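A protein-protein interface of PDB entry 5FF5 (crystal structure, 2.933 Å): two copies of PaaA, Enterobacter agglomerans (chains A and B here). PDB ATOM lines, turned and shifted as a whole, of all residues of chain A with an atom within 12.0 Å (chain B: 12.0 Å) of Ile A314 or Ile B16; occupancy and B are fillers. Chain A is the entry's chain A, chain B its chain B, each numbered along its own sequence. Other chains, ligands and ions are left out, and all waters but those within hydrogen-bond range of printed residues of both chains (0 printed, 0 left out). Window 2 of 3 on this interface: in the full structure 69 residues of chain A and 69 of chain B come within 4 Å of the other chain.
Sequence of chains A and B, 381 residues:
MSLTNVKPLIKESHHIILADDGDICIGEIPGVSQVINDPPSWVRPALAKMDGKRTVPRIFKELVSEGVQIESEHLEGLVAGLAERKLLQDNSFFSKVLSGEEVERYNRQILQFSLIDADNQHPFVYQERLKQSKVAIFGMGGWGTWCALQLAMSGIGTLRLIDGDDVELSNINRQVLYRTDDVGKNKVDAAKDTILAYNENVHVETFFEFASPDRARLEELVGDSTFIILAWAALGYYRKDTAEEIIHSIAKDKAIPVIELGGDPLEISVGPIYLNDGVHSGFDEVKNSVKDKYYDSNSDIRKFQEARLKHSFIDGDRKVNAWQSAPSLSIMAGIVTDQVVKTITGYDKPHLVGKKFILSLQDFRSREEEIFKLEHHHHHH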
ATOM      1  N   HIS A 311      41.908  25.317 -35.265  1.00  0.00           N
ATOM      2  CA  HIS A 311      42.129  26.501 -36.113  1.00  0.00           C
ATOM      3  C   HIS A 311      41.437  27.769 -35.604  1.00  0.00           C
ATOM      4  O   HIS A 311      41.427  28.064 -34.408  1.00  0.00           O
ATOM      5  CB  HIS A 311      41.657  26.233 -37.549  1.00  0.00           C
ATOM      6  N   SER A 312      40.876  28.531 -36.535  1.00  0.00           N
ATOM      7  CA  SER A 312      40.142  29.742 -36.179  1.00  0.00           C
ATOM      8  C   SER A 312      38.742  29.364 -35.698  1.00  0.00           C
ATOM      9  O   SER A 312      38.216  28.295 -36.039  1.00  0.00           O
ATOM     10  CB  SER A 312      40.072  30.713 -37.362  1.00  0.00           C
ATOM     11  N   PHE A 313      38.146  30.238 -34.893  1.00  0.00           N
ATOM     12  CA  PHE A 313      36.842  29.959 -34.293  1.00  0.00           C
ATOM     13  C   PHE A 313      35.803  31.000 -34.672  1.00  0.00           C
ATOM     14  O   PHE A 313      36.080  32.196 -34.712  1.00  0.00           O
ATOM     15  CB  PHE A 313      36.957  29.862 -32.759  1.00  0.00           C
ATOM     16  N   ILE A 314      34.588  30.528 -34.909  1.00  0.00           N
ATOM     17  CA  ILE A 314      33.490  31.393 -35.300  1.00  0.00           C
ATOM     18  C   ILE A 314      32.899  31.897 -34.001  1.00  0.00           C
ATOM     19  O   ILE A 314      31.691  31.817 -33.762  1.00  0.00           O
ATOM     20  CB  ILE A 314      32.442  30.631 -36.146  1.00  0.00           C
ATOM     21  CG1 ILE A 314      33.164  29.777 -37.200  1.00  0.00           C
ATOM     22  CG2 ILE A 314      31.403  31.598 -36.748  1.00  0.00           C
ATOM     23  CD1 ILE A 314      32.274  29.175 -38.228  1.00  0.00           C
ATOM     24  N   ASP A 315      33.786  32.451 -33.177  1.00  0.00           N
ATOM     25  CA  ASP A 315      33.490  32.748 -31.781  1.00  0.00           C
ATOM     26  C   ASP A 315      32.501  33.884 -31.569  1.00  0.00           C
ATOM     27  O   ASP A 315      31.625  33.802 -30.701  1.00  0.00           O
ATOM     28  CB  ASP A 315      34.796  33.079 -31.048  1.00  0.00           C
ATOM     29  N   GLY A 316      32.633  34.935 -32.362  1.00  0.00           N
ATOM     30  CA  GLY A 316      31.762  36.083 -32.220  1.00  0.00           C
ATOM     31  C   GLY A 316      32.170  36.880 -30.994  1.00  0.00           C
ATOM     32  O   GLY A 316      33.364  37.003 -30.695  1.00  0.00           O
ATOM     33  N   ASP A 317      31.189  37.412 -30.270  1.00  0.00           N
ATOM     34  CA  ASP A 317      31.487  38.268 -29.128  1.00  0.00           C
ATOM     35  C   ASP A 317      31.398  37.578 -27.761  1.00  0.00           C
ATOM     36  O   ASP A 317      31.646  38.225 -26.738  1.00  0.00           O
ATOM     37  CB  ASP A 317      30.557  39.480 -29.144  1.00  0.00           C
ATOM     38  N   ARG A 318      31.031  36.292 -27.728  1.00  0.00           N
ATOM     39  CA  ARG A 318      30.989  35.531 -26.463  1.00  0.00           C
ATOM     40  C   ARG A 318      32.389  35.075 -26.056  1.00  0.00           C
ATOM     41  O   ARG A 318      33.164  34.590 -26.879  1.00  0.00           O
ATOM     42  CB  ARG A 318      30.049  34.318 -26.564  1.00  0.00           C
ATOM     43  N   LYS A 319      32.708  35.219 -24.777  1.00  0.00           N
ATOM     44  CA  LYS A 319      34.027  34.821 -24.282  1.00  0.00           C
ATOM     45  C   LYS A 319      33.994  33.347 -23.850  1.00  0.00           C
ATOM     46  O   LYS A 319      33.221  32.973 -22.966  1.00  0.00           O
ATOM     47  CB  LYS A 319      34.472  35.719 -23.119  1.00  0.00           C
ATOM     48  N   VAL A 320      34.817  32.509 -24.484  1.00  0.00           N
ATOM     49  CA  VAL A 320      34.778  31.073 -24.212  1.00  0.00           C
ATOM     50  C   VAL A 320      35.814  30.727 -23.159  1.00  0.00           C
ATOM     51  O   VAL A 320      37.007  31.026 -23.301  1.00  0.00           O
ATOM     52  CB  VAL A 320      35.054  30.239 -25.474  1.00  0.00           C
ATOM     53  CG1 VAL A 320      35.237  28.759 -25.114  1.00  0.00           C
ATOM     54  CG2 VAL A 320      33.947  30.456 -26.501  1.00  0.00           C
ATOM     55  N   ASN A 321      35.336  30.097 -22.095  1.00  0.00           N
ATOM     56  CA  ASN A 321      36.146  29.859 -20.918  1.00  0.00           C
ATOM     57  C   ASN A 321      36.441  28.384 -20.653  1.00  0.00           C
ATOM     58  O   ASN A 321      35.817  27.499 -21.243  1.00  0.00           O
ATOM     59  CB  ASN A 321      35.438  30.470 -19.713  1.00  0.00           C
ATOM     60  CG  ASN A 321      35.422  31.991 -19.755  1.00  0.00           C
ATOM     61  OD1 ASN A 321      36.460  32.624 -19.912  1.00  0.00           O
ATOM     62  ND2 ASN A 321      34.232  32.582 -19.626  1.00  0.00           N
ATOM     63  N   TRP A 323      35.984  25.265 -18.380  1.00  0.00           N
ATOM     64  CA  TRP A 323      35.033  24.777 -17.365  1.00  0.00           C
ATOM     65  C   TRP A 323      35.682  23.807 -16.340  1.00  0.00           C
ATOM     66  O   TRP A 323      35.982  22.668 -16.663  1.00  0.00           O
ATOM     67  CB  TRP A 323      33.852  24.104 -18.065  1.00  0.00           C
ATOM     68  CG  TRP A 323      34.268  23.029 -19.019  1.00  0.00           C
ATOM     69  CD1 TRP A 323      34.891  23.189 -20.215  1.00  0.00           C
ATOM     70  CD2 TRP A 323      34.073  21.625 -18.852  1.00  0.00           C
ATOM     71  NE1 TRP A 323      35.112  21.967 -20.804  1.00  0.00           N
ATOM     72  CE2 TRP A 323      34.610  20.989 -19.987  1.00  0.00           C
ATOM     73  CE3 TRP A 323      33.508  20.841 -17.846  1.00  0.00           C
ATOM     74  CZ2 TRP A 323      34.599  19.610 -20.143  1.00  0.00           C
ATOM     75  CZ3 TRP A 323      33.494  19.480 -18.011  1.00  0.00           C
ATOM     76  CH2 TRP A 323      34.037  18.875 -19.146  1.00  0.00           C
ATOM     77  N   PRO B   8      20.071  33.798 -27.409  1.00  0.00           N
ATOM     78  CA  PRO B   8      21.053  32.729 -27.614  1.00  0.00           C
ATOM     79  C   PRO B   8      22.388  33.019 -26.945  1.00  0.00           C
ATOM     80  O   PRO B   8      23.191  33.806 -27.489  1.00  0.00           O
ATOM     81  CB  PRO B   8      21.239  32.696 -29.146  1.00  0.00           C
ATOM     82  CG  PRO B   8      19.996  33.192 -29.688  1.00  0.00           C
ATOM     83  CD  PRO B   8      19.478  34.228 -28.690  1.00  0.00           C
ATOM     84  N   LEU B   9      22.611  32.417 -25.777  1.00  0.00           N
ATOM     85  CA  LEU B   9      23.966  32.306 -25.258  1.00  0.00           C
ATOM     86  C   LEU B   9      24.486  30.911 -25.543  1.00  0.00           C
ATOM     87  O   LEU B   9      24.232  29.977 -24.785  1.00  0.00           O
ATOM     88  CB  LEU B   9      24.048  32.600 -23.761  1.00  0.00           C
ATOM     89  CG  LEU B   9      25.508  32.506 -23.291  1.00  0.00           C
ATOM     90  CD1 LEU B   9      26.433  33.104 -24.342  1.00  0.00           C
ATOM     91  CD2 LEU B   9      25.743  33.168 -21.946  1.00  0.00           C
ATOM     92  N   ILE B  10      25.190  30.767 -26.658  1.00  0.00           N
ATOM     93  CA  ILE B  10      25.938  29.552 -26.896  1.00  0.00           C
ATOM     94  C   ILE B  10      26.938  29.386 -25.756  1.00  0.00           C
ATOM     95  O   ILE B  10      28.015  30.009 -25.750  1.00  0.00           O
ATOM     96  CB  ILE B  10      26.668  29.560 -28.252  1.00  0.00           C
ATOM     97  CG1 ILE B  10      25.654  29.492 -29.396  1.00  0.00           C
ATOM     98  CG2 ILE B  10      27.622  28.390 -28.350  1.00  0.00           C
ATOM     99  CD1 ILE B  10      24.515  28.505 -29.165  1.00  0.00           C
ATOM    100  N   LYS B  11      26.511  28.563 -24.793  1.00  0.00           N
ATOM    101  CA  LYS B  11      27.257  28.076 -23.618  1.00  0.00           C
ATOM    102  C   LYS B  11      28.764  28.291 -23.631  1.00  0.00           C
ATOM    103  O   LYS B  11      29.491  27.674 -24.412  1.00  0.00           O
ATOM    104  CB  LYS B  11      26.949  26.583 -23.399  1.00  0.00           C
ATOM    105  CG  LYS B  11      25.768  26.344 -22.425  1.00  0.00           C
ATOM    106  CD  LYS B  11      25.349  24.887 -22.382  1.00  0.00           C
ATOM    107  CE  LYS B  11      24.070  24.695 -21.566  1.00  0.00           C
ATOM    108  NZ  LYS B  11      23.552  23.277 -21.554  1.00  0.00           N
ATOM    109  N   GLU B  12      29.214  29.202 -22.771  1.00  0.00           N
ATOM    110  CA  GLU B  12      30.573  29.737 -22.816  1.00  0.00           C
ATOM    111  C   GLU B  12      31.643  28.661 -22.623  1.00  0.00           C
ATOM    112  O   GLU B  12      32.839  28.954 -22.629  1.00  0.00           O
ATOM    113  CB  GLU B  12      30.733  30.842 -21.773  1.00  0.00           C
ATOM    114  CG  GLU B  12      29.524  31.766 -21.697  1.00  0.00           C
ATOM    115  CD  GLU B  12      29.847  33.150 -21.123  1.00  0.00           C
ATOM    116  OE1 GLU B  12      29.346  33.473 -20.013  1.00  0.00           O
ATOM    117  OE2 GLU B  12      30.575  33.926 -21.796  1.00  0.00           O
ATOM    118  N   SER B  13      31.197  27.426 -22.427  1.00  0.00           N
ATOM    119  CA  SER B  13      32.077  26.263 -22.401  1.00  0.00           C
ATOM    120  C   SER B  13      32.579  25.839 -23.782  1.00  0.00           C
ATOM    121  O   SER B  13      33.709  25.372 -23.924  1.00  0.00           O
ATOM    122  CB  SER B  13      31.349  25.085 -21.756  1.00  0.00           C
ATOM    123  OG  SER B  13      30.313  25.551 -20.917  1.00  0.00           O
ATOM    124  N   HIS B  14      31.733  25.998 -24.794  1.00  0.00           N
ATOM    125  CA  HIS B  14      32.011  25.457 -26.119  1.00  0.00           C
ATOM    126  C   HIS B  14      32.654  26.468 -27.065  1.00  0.00           C
ATOM    127  O   HIS B  14      32.221  27.624 -27.152  1.00  0.00           O
ATOM    128  CB  HIS B  14      30.726  24.956 -26.786  1.00  0.00           C
ATOM    129  CG  HIS B  14      29.900  24.050 -25.932  1.00  0.00           C
ATOM    130  ND1 HIS B  14      29.043  24.528 -24.964  1.00  0.00           N
ATOM    131  CD2 HIS B  14      29.787  22.701 -25.901  1.00  0.00           C
ATOM    132  CE1 HIS B  14      28.443  23.513 -24.370  1.00  0.00           C
ATOM    133  NE2 HIS B  14      28.874  22.393 -24.924  1.00  0.00           N
ATOM    134  N   HIS B  15      33.652  26.007 -27.809  1.00  0.00           N
ATOM    135  CA  HIS B  15      34.245  26.799 -28.880  1.00  0.00           C
ATOM    136  C   HIS B  15      33.445  26.509 -30.133  1.00  0.00           C
ATOM    137  O   HIS B  15      32.695  25.538 -30.161  1.00  0.00           O
ATOM    138  CB  HIS B  15      35.702  26.425 -29.109  1.00  0.00           C
ATOM    139  CG  HIS B  15      36.661  27.220 -28.296  1.00  0.00           C
ATOM    140  ND1 HIS B  15      36.553  28.586 -28.151  1.00  0.00           N
ATOM    141  CD2 HIS B  15      37.736  26.842 -27.566  1.00  0.00           C
ATOM    142  CE1 HIS B  15      37.533  29.017 -27.372  1.00  0.00           C
ATOM    143  NE2 HIS B  15      38.262  27.979 -27.005  1.00  0.00           N
ATOM    144  N   ILE B  16      33.550  27.346 -31.155  1.00  0.00           N
ATOM    145  CA  ILE B  16      33.004  26.935 -32.443  1.00  0.00           C
ATOM    146  C   ILE B  16      34.120  26.780 -33.487  1.00  0.00           C
ATOM    147  O   ILE B  16      34.711  25.695 -33.639  1.00  0.00           O
ATOM    148  CB  ILE B  16      31.939  27.903 -32.945  1.00  0.00           C
ATOM    149  CG1 ILE B  16      30.915  28.148 -31.832  1.00  0.00           C
ATOM    150  CG2 ILE B  16      31.298  27.322 -34.180  1.00  0.00           C
ATOM    151  CD1 ILE B  16      29.716  28.974 -32.217  1.00  0.00           C
ATOM    152  N   VAL B  79      18.175  27.278 -36.045  1.00  0.00           N
ATOM    153  CA  VAL B  79      19.410  27.146 -35.270  1.00  0.00           C
ATOM    154  C   VAL B  79      19.191  27.467 -33.786  1.00  0.00           C
ATOM    155  O   VAL B  79      19.684  26.740 -32.915  1.00  0.00           O
ATOM    156  CB  VAL B  79      20.540  28.054 -35.810  1.00  0.00           C
ATOM    157  N   ALA B  80      18.448  28.533 -33.490  1.00  0.00           N
ATOM    158  CA  ALA B  80      18.108  28.814 -32.098  1.00  0.00           C
ATOM    159  C   ALA B  80      17.409  27.609 -31.441  1.00  0.00           C
ATOM    160  O   ALA B  80      17.869  27.104 -30.417  1.00  0.00           O
ATOM    161  CB  ALA B  80      17.251  30.048 -31.994  1.00  0.00           C
ATOM    162  N   ALA B  83      19.034  24.338 -30.728  1.00  0.00           N
ATOM    163  CA  ALA B  83      19.951  24.568 -29.610  1.00  0.00           C
ATOM    164  C   ALA B  83      19.306  24.062 -28.309  1.00  0.00           C
ATOM    165  O   ALA B  83      19.950  24.016 -27.256  1.00  0.00           O
ATOM    166  CB  ALA B  83      20.326  26.045 -29.497  1.00  0.00           C
ATOM    167  N   LEU B  87      22.339  23.018 -25.585  1.00  0.00           N
ATOM    168  CA  LEU B  87      23.555  23.736 -25.949  1.00  0.00           C
ATOM    169  C   LEU B  87      23.394  25.250 -25.764  1.00  0.00           C
ATOM    170  O   LEU B  87      24.325  26.022 -26.044  1.00  0.00           O
ATOM    171  CB  LEU B  87      23.939  23.435 -27.393  1.00  0.00           C
ATOM    172  CG  LEU B  87      24.694  22.124 -27.575  1.00  0.00           C
ATOM    173  CD1 LEU B  87      25.352  22.052 -28.952  1.00  0.00           C
ATOM    174  CD2 LEU B  87      25.718  21.952 -26.466  1.00  0.00           C
ATOM    175  N   LEU B  88      22.191  25.675 -25.376  1.00  0.00           N
ATOM    176  CA  LEU B  88      21.911  27.097 -25.239  1.00  0.00           C
ATOM    177  C   LEU B  88      21.523  27.551 -23.838  1.00  0.00           C
ATOM    178  O   LEU B  88      20.779  26.876 -23.118  1.00  0.00           O
ATOM    179  CB  LEU B  88      20.798  27.511 -26.215  1.00  0.00           C
ATOM    180  N   GLN B  89      22.043  28.712 -23.464  1.00  0.00           N
ATOM    181  CA  GLN B  89      21.729  29.342 -22.189  1.00  0.00           C
ATOM    182  C   GLN B  89      20.621  30.373 -22.394  1.00  0.00           C
ATOM    183  O   GLN B  89      20.343  30.777 -23.528  1.00  0.00           O
ATOM    184  CB  GLN B  89      22.965  29.999 -21.576  1.00  0.00           C
ATOM    185  CG  GLN B  89      22.991  29.932 -20.061  1.00  0.00           C
ATOM    186  CD  GLN B  89      23.365  28.544 -19.547  1.00  0.00           C
ATOM    187  OE1 GLN B  89      24.537  28.275 -19.253  1.00  0.00           O
ATOM    188  NE2 GLN B  89      22.371  27.654 -19.449  1.00  0.00           N
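Hydrophobic or aromatic side chains of chain B that line the printed part of chain A: His B15 and Ile B16. Hydrophobic or aromatic side chains of chain A that line the printed part of chain B: Val A320.
The backbone carbonyl oxygen (O) of Glu B12 lies within hydrogen-bond range of the backbone NH (N) of Asn A321. OE2 of Glu B12 sits close to O of Lys A319 (3.0 Å).
No position is printed for both chains. Of the 7 pairs that touch across the chains among the printed residues, none has its exchanged pair printed and touching as well.
A ring nitrogen (ND1) of His B14 lies within hydrogen-bond range of the backbone carbonyl oxygen (O) of Lys B11 (3.2 Å).
No residue of chain B comes within 4 Å of Phe A313. Of chain B, only Ile B16 (3.8 Å) comes within 4 Å of Ile A314. Of the printed residues of chain B, Lys A319 touches Glu B12 (3.0 Å). Printed residues of chain B within 4 Å of Val A320: Glu B12, Ser B13, His B14 and His B15. Printed residues of chain B within 4 Å of Asn A321: Glu B12 (2.8 Å). Of the printed residues of chain A, Ser B13 touches Val A320 (3.9 Å). Printed residues of chain A within 4 Å of His B14: Val A320. Ile B16 touches one residue of chain A. The nearest residue of chain B that does not touch Ile A314 is His B15 (6.3 Å). The nearest printed residue of chain A that does not touch Glu B12 is Arg A318 (4.8 Å).
Among the printed residues, merely in contact across the chains: Ile A314 with Ile B16 (3.8 Å), Val A320 with Glu B12 (3.3 Å), Val A320 with Ser B13 (3.9 Å), Val A320 with His B14 (3.4 Å) and Val A320 with His B15 (3.2 Å).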
